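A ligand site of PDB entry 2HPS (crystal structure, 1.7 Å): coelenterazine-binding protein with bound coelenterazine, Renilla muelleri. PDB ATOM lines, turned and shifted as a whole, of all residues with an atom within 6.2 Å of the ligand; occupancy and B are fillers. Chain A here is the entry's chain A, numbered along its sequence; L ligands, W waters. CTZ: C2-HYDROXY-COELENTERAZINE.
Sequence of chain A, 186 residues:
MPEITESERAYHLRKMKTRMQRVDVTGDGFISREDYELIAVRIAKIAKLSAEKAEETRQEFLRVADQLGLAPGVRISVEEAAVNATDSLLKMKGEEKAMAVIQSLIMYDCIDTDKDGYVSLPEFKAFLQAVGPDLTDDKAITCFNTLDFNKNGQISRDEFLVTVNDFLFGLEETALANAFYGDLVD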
ATOM      1  N   ARG A  19       4.332   1.537 -12.549  1.00  0.00           N
ATOM      2  CA  ARG A  19       5.133   1.640 -13.775  1.00  0.00           C
ATOM      3  C   ARG A  19       6.161   2.778 -13.633  1.00  0.00           C
ATOM      4  O   ARG A  19       7.321   2.609 -13.959  1.00  0.00           O
ATOM      5  CB  ARG A  19       4.201   1.940 -14.949  1.00  0.00           C
ATOM      6  CG  ARG A  19       4.914   2.195 -16.264  1.00  0.00           C
ATOM      7  CD  ARG A  19       3.868   2.562 -17.327  1.00  0.00           C
ATOM      8  NE  ARG A  19       4.500   3.209 -18.483  1.00  0.00           N
ATOM      9  CZ  ARG A  19       3.859   3.987 -19.368  1.00  0.00           C
ATOM     10  NH1 ARG A  19       2.551   4.211 -19.261  1.00  0.00           N
ATOM     11  NH2 ARG A  19       4.536   4.523 -20.366  1.00  0.00           N
ATOM     12  N   MET A  20       5.724   3.914 -13.125  1.00  0.00           N
ATOM     13  CA  MET A  20       6.608   5.052 -13.061  1.00  0.00           C
ATOM     14  C   MET A  20       7.708   4.868 -12.034  1.00  0.00           C
ATOM     15  O   MET A  20       8.831   5.379 -12.207  1.00  0.00           O
ATOM     16  CB  MET A  20       5.822   6.333 -12.802  1.00  0.00           C
ATOM     17  CG  MET A  20       4.870   6.719 -13.921  1.00  0.00           C
ATOM     18  SD  MET A  20       5.855   7.093 -15.574  1.00  0.00           S
ATOM     19  CE  MET A  20       5.769   5.534 -16.557  1.00  0.00           C
ATOM     20  N   ARG A  22       9.323   2.296 -11.612  1.00  0.00           N
ATOM     21  CA  ARG A  22      10.387   1.574 -12.307  1.00  0.00           C
ATOM     22  C   ARG A  22      11.358   2.508 -13.010  1.00  0.00           C
ATOM     23  O   ARG A  22      12.506   2.136 -13.262  1.00  0.00           O
ATOM     24  CB  ARG A  22       9.804   0.548 -13.295  1.00  0.00           C
ATOM     25  CG  ARG A  22       8.993  -0.563 -12.636  1.00  0.00           C
ATOM     26  CD  ARG A  22       9.826  -1.339 -11.618  1.00  0.00           C
ATOM     27  NE  ARG A  22      11.121  -1.737 -12.170  1.00  0.00           N
ATOM     28  CZ  ARG A  22      12.125  -2.242 -11.449  1.00  0.00           C
ATOM     29  NH1 ARG A  22      13.270  -2.548 -12.050  1.00  0.00           N
ATOM     30  NH2 ARG A  22      11.993  -2.439 -10.140  1.00  0.00           N
ATOM     31  N   VAL A  23      10.903   3.722 -13.306  1.00  0.00           N
ATOM     32  CA  VAL A  23      11.749   4.723 -13.940  1.00  0.00           C
ATOM     33  C   VAL A  23      12.633   5.389 -12.866  1.00  0.00           C
ATOM     34  O   VAL A  23      13.736   5.873 -13.144  1.00  0.00           O
ATOM     35  CB  VAL A  23      10.899   5.743 -14.750  1.00  0.00           C
ATOM     36  CG1 VAL A  23      11.797   6.727 -15.526  1.00  0.00           C
ATOM     37  CG2 VAL A  23       9.970   5.011 -15.733  1.00  0.00           C
ATOM     38  N   TYR A  36      14.272   7.836 -18.232  1.00  0.00           N
ATOM     39  CA  TYR A  36      13.513   7.051 -19.194  1.00  0.00           C
ATOM     40  C   TYR A  36      14.405   6.506 -20.319  1.00  0.00           C
ATOM     41  O   TYR A  36      14.335   5.329 -20.680  1.00  0.00           O
ATOM     42  CB  TYR A  36      12.318   7.867 -19.709  1.00  0.00           C
ATOM     43  CG  TYR A  36      11.105   7.031 -20.052  1.00  0.00           C
ATOM     44  CD1 TYR A  36      10.584   6.090 -19.136  1.00  0.00           C
ATOM     45  CD2 TYR A  36      10.449   7.190 -21.291  1.00  0.00           C
ATOM     46  CE1 TYR A  36       9.459   5.317 -19.468  1.00  0.00           C
ATOM     47  CE2 TYR A  36       9.336   6.435 -21.610  1.00  0.00           C
ATOM     48  CZ  TYR A  36       8.844   5.496 -20.703  1.00  0.00           C
ATOM     49  OH  TYR A  36       7.734   4.759 -21.050  1.00  0.00           O
ATOM     50  N   ILE A  39      16.369   3.294 -19.578  1.00  0.00           N
ATOM     51  CA  ILE A  39      15.652   2.043 -19.884  1.00  0.00           C
ATOM     52  C   ILE A  39      15.874   1.627 -21.340  1.00  0.00           C
ATOM     53  O   ILE A  39      16.230   0.476 -21.613  1.00  0.00           O
ATOM     54  CB  ILE A  39      14.151   2.182 -19.553  1.00  0.00           C
ATOM     55  CG1 ILE A  39      14.002   2.355 -18.043  1.00  0.00           C
ATOM     56  CG2 ILE A  39      13.366   0.950 -20.075  1.00  0.00           C
ATOM     57  CD1 ILE A  39      12.640   2.779 -17.601  1.00  0.00           C
ATOM     58  N   ILE A  43      17.721  -1.731 -22.764  1.00  0.00           N
ATOM     59  CA  ILE A  43      17.026  -2.585 -23.740  1.00  0.00           C
ATOM     60  C   ILE A  43      17.948  -2.886 -24.925  1.00  0.00           C
ATOM     61  O   ILE A  43      18.140  -4.047 -25.317  1.00  0.00           O
ATOM     62  CB  ILE A  43      15.684  -1.943 -24.212  1.00  0.00           C
ATOM     63  CG1 ILE A  43      14.633  -2.024 -23.098  1.00  0.00           C
ATOM     64  CG2 ILE A  43      15.148  -2.641 -25.499  1.00  0.00           C
ATOM     65  CD1 ILE A  43      13.424  -1.114 -23.298  1.00  0.00           C
ATOM     66  N   PHE A  61      10.863   5.686 -26.924  1.00  0.00           N
ATOM     67  CA  PHE A  61      10.845   6.124 -25.525  1.00  0.00           C
ATOM     68  C   PHE A  61      10.725   7.637 -25.350  1.00  0.00           C
ATOM     69  O   PHE A  61      10.024   8.104 -24.461  1.00  0.00           O
ATOM     70  CB  PHE A  61      12.045   5.561 -24.744  1.00  0.00           C
ATOM     71  CG  PHE A  61      11.796   4.178 -24.199  1.00  0.00           C
ATOM     72  CD1 PHE A  61      11.687   3.085 -25.062  1.00  0.00           C
ATOM     73  CD2 PHE A  61      11.631   3.981 -22.824  1.00  0.00           C
ATOM     74  CE1 PHE A  61      11.425   1.782 -24.546  1.00  0.00           C
ATOM     75  CE2 PHE A  61      11.363   2.713 -22.310  1.00  0.00           C
ATOM     76  CZ  PHE A  61      11.279   1.605 -23.170  1.00  0.00           C
ATOM     77  N   VAL A  64       7.035   8.687 -26.010  1.00  0.00           N
ATOM     78  CA  VAL A  64       6.254   8.390 -24.798  1.00  0.00           C
ATOM     79  C   VAL A  64       6.642   9.345 -23.659  1.00  0.00           C
ATOM     80  O   VAL A  64       5.768   9.850 -22.967  1.00  0.00           O
ATOM     81  CB  VAL A  64       6.351   6.891 -24.432  1.00  0.00           C
ATOM     82  CG1 VAL A  64       5.594   6.580 -23.141  1.00  0.00           C
ATOM     83  CG2 VAL A  64       5.797   6.043 -25.583  1.00  0.00           C
ATOM     84  N   LEU A  68       4.352  11.608 -21.068  1.00  0.00           N
ATOM     85  CA  LEU A  68       4.457  11.456 -19.618  1.00  0.00           C
ATOM     86  C   LEU A  68       4.797  12.783 -18.926  1.00  0.00           C
ATOM     87  O   LEU A  68       4.788  12.868 -17.702  1.00  0.00           O
ATOM     88  CB  LEU A  68       5.482  10.386 -19.251  1.00  0.00           C
ATOM     89  CG  LEU A  68       5.113   8.978 -19.779  1.00  0.00           C
ATOM     90  CD1 LEU A  68       6.250   7.988 -19.516  1.00  0.00           C
ATOM     91  CD2 LEU A  68       3.780   8.521 -19.167  1.00  0.00           C
ATOM     92  N   GLN A 103       5.539   0.653 -28.148  1.00  0.00           N
ATOM     93  CA  GLN A 103       6.658   0.551 -27.232  1.00  0.00           C
ATOM     94  C   GLN A 103       6.807  -0.875 -26.678  1.00  0.00           C
ATOM     95  O   GLN A 103       7.909  -1.441 -26.645  1.00  0.00           O
ATOM     96  CB  GLN A 103       6.452   1.548 -26.103  1.00  0.00           C
ATOM     97  CG  GLN A 103       7.642   1.806 -25.242  1.00  0.00           C
ATOM     98  CD  GLN A 103       7.295   2.760 -24.108  1.00  0.00           C
ATOM     99  OE1 GLN A 103       6.113   2.959 -23.779  1.00  0.00           O
ATOM    100  NE2 GLN A 103       8.311   3.359 -23.515  1.00  0.00           N
ATOM    101  N   MET A 107       9.700  -3.851 -27.218  1.00  0.00           N
ATOM    102  CA  MET A 107      10.272  -4.645 -26.134  1.00  0.00           C
ATOM    103  C   MET A 107      10.088  -6.135 -26.360  1.00  0.00           C
ATOM    104  O   MET A 107      11.026  -6.898 -26.157  1.00  0.00           O
ATOM    105  CB  MET A 107       9.722  -4.231 -24.777  1.00  0.00           C
ATOM    106  CG  MET A 107      10.024  -2.785 -24.491  1.00  0.00           C
ATOM    107  SD  MET A 107       9.369  -2.260 -22.726  1.00  0.00           S
ATOM    108  CE  MET A 107      10.159  -3.148 -21.857  1.00  0.00           C
ATOM    109  N   ILE A 111      12.953  -9.274 -26.562  1.00  0.00           N
ATOM    110  CA  ILE A 111      12.981 -10.532 -25.798  1.00  0.00           C
ATOM    111  C   ILE A 111      13.079 -11.741 -26.745  1.00  0.00           C
ATOM    112  O   ILE A 111      13.774 -12.734 -26.446  1.00  0.00           O
ATOM    113  CB  ILE A 111      11.705 -10.719 -24.934  1.00  0.00           C
ATOM    114  CG1 ILE A 111      11.443  -9.471 -24.068  1.00  0.00           C
ATOM    115  CG2 ILE A 111      11.827 -11.960 -24.041  1.00  0.00           C
ATOM    116  CD1 ILE A 111      10.085  -9.501 -23.339  1.00  0.00           C
ATOM    117  N   PHE A 124      12.950 -14.255 -21.311  1.00  0.00           N
ATOM    118  CA  PHE A 124      12.142 -13.288 -20.573  1.00  0.00           C
ATOM    119  C   PHE A 124      12.884 -12.822 -19.325  1.00  0.00           C
ATOM    120  O   PHE A 124      12.989 -11.617 -19.080  1.00  0.00           O
ATOM    121  CB  PHE A 124      10.842 -13.996 -20.213  1.00  0.00           C
ATOM    122  CG  PHE A 124       9.843 -13.161 -19.473  1.00  0.00           C
ATOM    123  CD1 PHE A 124       8.728 -12.641 -20.146  1.00  0.00           C
ATOM    124  CD2 PHE A 124       9.964 -12.968 -18.099  1.00  0.00           C
ATOM    125  CE1 PHE A 124       7.757 -11.900 -19.432  1.00  0.00           C
ATOM    126  CE2 PHE A 124       9.004 -12.237 -17.398  1.00  0.00           C
ATOM    127  CZ  PHE A 124       7.904 -11.721 -18.054  1.00  0.00           C
ATOM    128  N   PHE A 127      15.925 -10.587 -20.177  1.00  0.00           N
ATOM    129  CA  PHE A 127      15.468  -9.254 -20.569  1.00  0.00           C
ATOM    130  C   PHE A 127      14.995  -8.425 -19.367  1.00  0.00           C
ATOM    131  O   PHE A 127      15.424  -7.290 -19.157  1.00  0.00           O
ATOM    132  CB  PHE A 127      14.379  -9.322 -21.649  1.00  0.00           C
ATOM    133  CG  PHE A 127      13.834  -7.964 -22.029  1.00  0.00           C
ATOM    134  CD1 PHE A 127      14.416  -7.233 -23.049  1.00  0.00           C
ATOM    135  CD2 PHE A 127      12.751  -7.418 -21.334  1.00  0.00           C
ATOM    136  CE1 PHE A 127      13.924  -5.974 -23.382  1.00  0.00           C
ATOM    137  CE2 PHE A 127      12.250  -6.170 -21.667  1.00  0.00           C
ATOM    138  CZ  PHE A 127      12.851  -5.447 -22.694  1.00  0.00           C
ATOM    139  N   LEU A 128      14.131  -9.024 -18.560  1.00  0.00           N
ATOM    140  CA  LEU A 128      13.566  -8.321 -17.431  1.00  0.00           C
ATOM    141  C   LEU A 128      14.628  -7.907 -16.419  1.00  0.00           C
ATOM    142  O   LEU A 128      14.571  -6.809 -15.859  1.00  0.00           O
ATOM    143  CB  LEU A 128      12.481  -9.166 -16.773  1.00  0.00           C
ATOM    144  CG  LEU A 128      11.760  -8.483 -15.625  1.00  0.00           C
ATOM    145  CD1 LEU A 128      11.161  -7.121 -16.072  1.00  0.00           C
ATOM    146  CD2 LEU A 128      10.660  -9.418 -15.095  1.00  0.00           C
ATOM    147  N   VAL A 131      16.644  -4.861 -17.835  1.00  0.00           N
ATOM    148  CA  VAL A 131      15.976  -3.552 -17.650  1.00  0.00           C
ATOM    149  C   VAL A 131      15.848  -3.244 -16.167  1.00  0.00           C
ATOM    150  O   VAL A 131      15.932  -2.081 -15.767  1.00  0.00           O
ATOM    151  CB  VAL A 131      14.599  -3.424 -18.393  1.00  0.00           C
ATOM    152  CG1 VAL A 131      14.780  -3.783 -19.882  1.00  0.00           C
ATOM    153  CG2 VAL A 131      13.542  -4.267 -17.760  1.00  0.00           C
ATOM    154  N   GLY A 132      15.699  -4.299 -15.361  1.00  0.00           N
ATOM    155  CA  GLY A 132      15.537  -4.162 -13.911  1.00  0.00           C
ATOM    156  C   GLY A 132      16.473  -5.078 -13.140  1.00  0.00           C
ATOM    157  O   GLY A 132      16.045  -6.100 -12.589  1.00  0.00           O
ATOM    158  N   LEU A 135      15.772  -6.637  -9.724  1.00  0.00           N
ATOM    159  CA  LEU A 135      14.735  -7.674  -9.598  1.00  0.00           C
ATOM    160  C   LEU A 135      15.312  -9.069  -9.361  1.00  0.00           C
ATOM    161  O   LEU A 135      16.109  -9.559 -10.164  1.00  0.00           O
ATOM    162  CB  LEU A 135      13.848  -7.695 -10.848  1.00  0.00           C
ATOM    163  CG  LEU A 135      13.025  -6.419 -11.097  1.00  0.00           C
ATOM    164  CD1 LEU A 135      12.313  -6.467 -12.451  1.00  0.00           C
ATOM    165  CD2 LEU A 135      12.020  -6.175  -9.969  1.00  0.00           C
ATOM    166  N   LYS A 139      11.151 -12.707  -8.381  1.00  0.00           N
ATOM    167  CA  LYS A 139      10.271 -11.748  -9.014  1.00  0.00           C
ATOM    168  C   LYS A 139      10.150 -11.930 -10.521  1.00  0.00           C
ATOM    169  O   LYS A 139       9.046 -11.848 -11.067  1.00  0.00           O
ATOM    170  CB  LYS A 139      10.644 -10.302  -8.651  1.00  0.00           C
ATOM    171  CG  LYS A 139      10.287  -9.963  -7.205  1.00  0.00           C
ATOM    172  CD  LYS A 139      10.704  -8.539  -6.864  1.00  0.00           C
ATOM    173  CE  LYS A 139      10.896  -8.337  -5.342  1.00  0.00           C
ATOM    174  NZ  LYS A 139       9.773  -8.888  -4.535  1.00  0.00           N
ATOM    175  N   ALA A 140      11.275 -12.177 -11.186  1.00  0.00           N
ATOM    176  CA  ALA A 140      11.259 -12.293 -12.654  1.00  0.00           C
ATOM    177  C   ALA A 140      10.485 -13.537 -13.078  1.00  0.00           C
ATOM    178  O   ALA A 140       9.712 -13.505 -14.024  1.00  0.00           O
ATOM    179  CB  ALA A 140      12.668 -12.323 -13.198  1.00  0.00           C
ATOM    180  N   CYS A 143       6.742 -13.300 -12.487  1.00  0.00           N
ATOM    181  CA  CYS A 143       6.164 -12.481 -13.534  1.00  0.00           C
ATOM    182  C   CYS A 143       5.903 -13.311 -14.817  1.00  0.00           C
ATOM    183  O   CYS A 143       4.780 -13.307 -15.380  1.00  0.00           O
ATOM    184  CB  CYS A 143       7.081 -11.282 -13.816  1.00  0.00           C
ATOM    185  SG  CYS A 143       6.407 -10.071 -15.011  1.00  0.00           S
ATOM    186  N   LEU A 147       2.262 -14.272 -16.661  1.00  0.00           N
ATOM    187  CA  LEU A 147       2.007 -13.818 -18.019  1.00  0.00           C
ATOM    188  C   LEU A 147       1.839 -14.970 -19.010  1.00  0.00           C
ATOM    189  O   LEU A 147       1.232 -14.812 -20.066  1.00  0.00           O
ATOM    190  CB  LEU A 147       3.119 -12.884 -18.492  1.00  0.00           C
ATOM    191  CG  LEU A 147       2.804 -11.392 -18.331  1.00  0.00           C
ATOM    192  CD1 LEU A 147       2.549 -11.013 -16.906  1.00  0.00           C
ATOM    193  CD2 LEU A 147       3.989 -10.595 -18.847  1.00  0.00           C
ATOM    194  N   PHE A 160       1.247 -11.804 -24.909  1.00  0.00           N
ATOM    195  CA  PHE A 160       1.932 -10.654 -24.318  1.00  0.00           C
ATOM    196  C   PHE A 160       1.078  -9.397 -24.531  1.00  0.00           C
ATOM    197  O   PHE A 160       0.860  -8.609 -23.601  1.00  0.00           O
ATOM    198  CB  PHE A 160       3.319 -10.508 -24.913  1.00  0.00           C
ATOM    199  CG  PHE A 160       4.172  -9.438 -24.249  1.00  0.00           C
ATOM    200  CD1 PHE A 160       4.770  -9.688 -23.019  1.00  0.00           C
ATOM    201  CD2 PHE A 160       4.382  -8.201 -24.883  1.00  0.00           C
ATOM    202  CE1 PHE A 160       5.581  -8.694 -22.411  1.00  0.00           C
ATOM    203  CE2 PHE A 160       5.197  -7.211 -24.281  1.00  0.00           C
ATOM    204  CZ  PHE A 160       5.784  -7.480 -23.046  1.00  0.00           C
ATOM    205  N   ALA A 179       0.281  -8.119 -12.169  1.00  0.00           N
ATOM    206  CA  ALA A 179       1.575  -8.814 -12.190  1.00  0.00           C
ATOM    207  C   ALA A 179       2.606  -8.205 -13.139  1.00  0.00           C
ATOM    208  O   ALA A 179       3.818  -8.353 -12.910  1.00  0.00           O
ATOM    209  CB  ALA A 179       1.376 -10.269 -12.534  1.00  0.00           C
ATOM    210  N   PHE A 180       2.131  -7.540 -14.192  1.00  0.00           N
ATOM    211  CA  PHE A 180       2.993  -7.078 -15.309  1.00  0.00           C
ATOM    212  C   PHE A 180       4.192  -6.242 -14.855  1.00  0.00           C
ATOM    213  O   PHE A 180       5.315  -6.451 -15.350  1.00  0.00           O
ATOM    214  CB  PHE A 180       2.146  -6.299 -16.327  1.00  0.00           C
ATOM    215  CG  PHE A 180       2.854  -6.000 -17.650  1.00  0.00           C
ATOM    216  CD1 PHE A 180       3.747  -6.903 -18.226  1.00  0.00           C
ATOM    217  CD2 PHE A 180       2.549  -4.823 -18.358  1.00  0.00           C
ATOM    218  CE1 PHE A 180       4.362  -6.597 -19.451  1.00  0.00           C
ATOM    219  CE2 PHE A 180       3.155  -4.527 -19.583  1.00  0.00           C
ATOM    220  CZ  PHE A 180       4.065  -5.427 -20.131  1.00  0.00           C
ATOM    221  N   TYR A 181       3.928  -5.304 -13.930  1.00  0.00           N
ATOM    222  CA  TYR A 181       4.951  -4.459 -13.326  1.00  0.00           C
ATOM    223  C   TYR A 181       5.185  -4.789 -11.855  1.00  0.00           C
ATOM    224  O   TYR A 181       5.613  -3.935 -11.050  1.00  0.00           O
ATOM    225  CB  TYR A 181       4.556  -2.984 -13.516  1.00  0.00           C
ATOM    226  CG  TYR A 181       5.000  -2.438 -14.848  1.00  0.00           C
ATOM    227  CD1 TYR A 181       6.229  -1.793 -14.988  1.00  0.00           C
ATOM    228  CD2 TYR A 181       4.188  -2.580 -15.983  1.00  0.00           C
ATOM    229  CE1 TYR A 181       6.640  -1.296 -16.218  1.00  0.00           C
ATOM    230  CE2 TYR A 181       4.600  -2.073 -17.235  1.00  0.00           C
ATOM    231  CZ  TYR A 181       5.831  -1.432 -17.324  1.00  0.00           C
ATOM    232  OH  TYR A 181       6.243  -0.936 -18.536  1.00  0.00           O
ATOM    233  N   GLY A 182       4.927  -6.054 -11.505  1.00  0.00           N
ATOM    234  CA  GLY A 182       5.057  -6.528 -10.101  1.00  0.00           C
ATOM    235  C   GLY A 182       3.971  -6.002  -9.175  1.00  0.00           C
ATOM    236  O   GLY A 182       2.973  -5.430  -9.619  1.00  0.00           O
ATOM    237  N   ASP A 183       4.168  -6.217  -7.874  1.00  0.00           N
ATOM    238  CA  ASP A 183       3.133  -5.866  -6.905  1.00  0.00           C
ATOM    239  C   ASP A 183       2.899  -4.368  -6.957  1.00  0.00           C
ATOM    240  O   ASP A 183       3.849  -3.573  -6.903  1.00  0.00           O
ATOM    241  CB  ASP A 183       3.546  -6.285  -5.485  1.00  0.00           C
ATOM    242  CG  ASP A 183       3.648  -7.797  -5.304  1.00  0.00           C
ATOM    243  OD1 ASP A 183       3.037  -8.567  -6.088  1.00  0.00           O
ATOM    244  OD2 ASP A 183       4.325  -8.193  -4.338  1.00  0.00           O
HETATM  245  N1  CTZ L   1       9.327  -2.719 -17.695  1.00  0.00           N
HETATM  246  C2  CTZ L   1      10.356  -1.916 -17.286  1.00  0.00           C
HETATM  247  C3  CTZ L   1      10.580  -2.351 -15.908  1.00  0.00           C
HETATM  248  N4  CTZ L   1       9.745  -3.338 -15.570  1.00  0.00           N
HETATM  249  C5  CTZ L   1       9.596  -4.031 -14.421  1.00  0.00           C
HETATM  250  C6  CTZ L   1       8.607  -5.004 -14.351  1.00  0.00           C
HETATM  251  N7  CTZ L   1       7.814  -5.272 -15.415  1.00  0.00           N
HETATM  252  C8  CTZ L   1       7.949  -4.604 -16.588  1.00  0.00           C
HETATM  253  C9  CTZ L   1       8.980  -3.544 -16.660  1.00  0.00           C
HETATM  254  C10 CTZ L   1      11.037  -0.845 -18.103  1.00  0.00           C
HETATM  255  C11 CTZ L   1       9.989   0.197 -18.407  1.00  0.00           C
HETATM  256  C12 CTZ L   1       9.564   0.374 -19.721  1.00  0.00           C
HETATM  257  C13 CTZ L   1       8.586   1.312 -20.037  1.00  0.00           C
HETATM  258  C14 CTZ L   1       8.046   2.091 -19.008  1.00  0.00           C
HETATM  259  C15 CTZ L   1       8.464   1.911 -17.682  1.00  0.00           C
HETATM  260  C16 CTZ L   1       9.439   0.965 -17.378  1.00  0.00           C
HETATM  261  O17 CTZ L   1       7.101   3.009 -19.309  1.00  0.00           O
HETATM  262  O18 CTZ L   1      11.457  -1.859 -15.089  1.00  0.00           O
HETATM  263  C19 CTZ L   1       8.456  -5.794 -13.110  1.00  0.00           C
HETATM  264  C20 CTZ L   1       8.663  -5.223 -11.854  1.00  0.00           C
HETATM  265  C21 CTZ L   1       8.518  -5.997 -10.699  1.00  0.00           C
HETATM  266  C22 CTZ L   1       8.183  -7.357 -10.803  1.00  0.00           C
HETATM  267  C23 CTZ L   1       7.989  -7.939 -12.055  1.00  0.00           C
HETATM  268  C24 CTZ L   1       8.129  -7.161 -13.203  1.00  0.00           C
HETATM  269  O25 CTZ L   1       8.062  -8.085  -9.664  1.00  0.00           O
HETATM  270  C26 CTZ L   1       7.056  -4.854 -17.784  1.00  0.00           C
HETATM  271  C27 CTZ L   1       7.631  -5.998 -18.585  1.00  0.00           C
HETATM  272  C28 CTZ L   1       8.142  -5.806 -19.869  1.00  0.00           C
HETATM  273  C29 CTZ L   1       8.649  -6.897 -20.570  1.00  0.00           C
HETATM  274  C30 CTZ L   1       8.660  -8.176 -19.974  1.00  0.00           C
HETATM  275  C31 CTZ L   1       8.128  -8.358 -18.699  1.00  0.00           C
HETATM  276  C32 CTZ L   1       7.614  -7.269 -18.004  1.00  0.00           C
HETATM  277  O   HOH W   1       6.787  -7.321  -7.175  1.00  0.00           O
HETATM  278  O   HOH W   2      13.743  -0.849 -14.539  1.00  0.00           O
HETATM  279  O   HOH W   3       6.977 -10.523  -9.887  1.00  0.00           O
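The side-chain hydroxyl (OH) of Tyr 36 lies within hydrogen-bond range of an oxygen (O17) of the ligand (2.5 Å).
O17 of the ligand lies within hydrogen-bond range of NE of Arg 19, 2.7 Å away.
NE of Arg 22 sits at hydrogen-bond distance from O18 of the ligand, 2.9 Å away.
The side-chain amide nitrogen (NE2) of Gln 103 lies within hydrogen-bond range of the side-chain hydroxyl (OH) of Tyr 36 (2.9 Å).
NH2 of Arg 19 is in hydrogen-bond range of OH of Tyr 36 (3.3 Å).
SG of Cys 143 sits at hydrogen-bond distance from O of Phe 180.
SG of Cys 143 lies within hydrogen-bond range of O of Ala 179.
The backbone carbonyl oxygen of Phe 180 sits close to a nitrogen (N7) of the ligand (2.8 Å).
CE of Met 20 touches O17 of the ligand, at 3.97 Å.
Val 23 touches the ligand.
Ile 39 touches the ligand (CG2 to C10, 3.5 Å).
CE2 of Phe 61 touches C13 of the ligand, at 3.9 Å.
Met 107 touches the ligand (CE to C28, 3.9 Å).
Ile 111 touches the ligand (CD1 to C30, 3.9 Å).
Phe 124 touches the ligand.
Phe 127 touches the ligand (CE2 to C29, 3.8 Å).
CD1 of Leu 128 touches C6 of the ligand, at 3.7 Å.
Val 131 touches the ligand.
Leu 135 touches the ligand.
Lys 139 touches the ligand (CB to O25, 3.6 Å).
Cys 143 touches the ligand.
Phe 160 touches the ligand (CZ to C29, 3.8 Å).
Tyr 181 touches the ligand (CE1 to C9, 3.3 Å).
CA of Gly 182 touches C22 of the ligand (3.3 Å).
Hydrophobic or aromatic side chains that line the ligand: Met 20, Val 23, Tyr 36, Ile 39, Phe 61, Met 107, Ile 111, Phe 124, Phe 127, Leu 128, Val 131, Leu 135, Phe 160, Phe 180 and Tyr 181.
Of the 29 residues printed, 20 come within 4 Å of the ligand.
The nearest printed residue that does not touch the ligand is Gln 103 (4.05 Å).
Water W2 lies within hydrogen-bond range of an oxygen (O18) of the ligand (2.6 Å), the backbone carbonyl oxygen of Val 131 (2.8 Å) and the guanidinium group of Arg 22 (3.1 Å).
Water W3 bridges O25 of the ligand (2.7 Å) and O of Lys 139 (2.7 Å).
Water W1 lies within hydrogen-bond range of O25 of the ligand and N of Asp 183.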
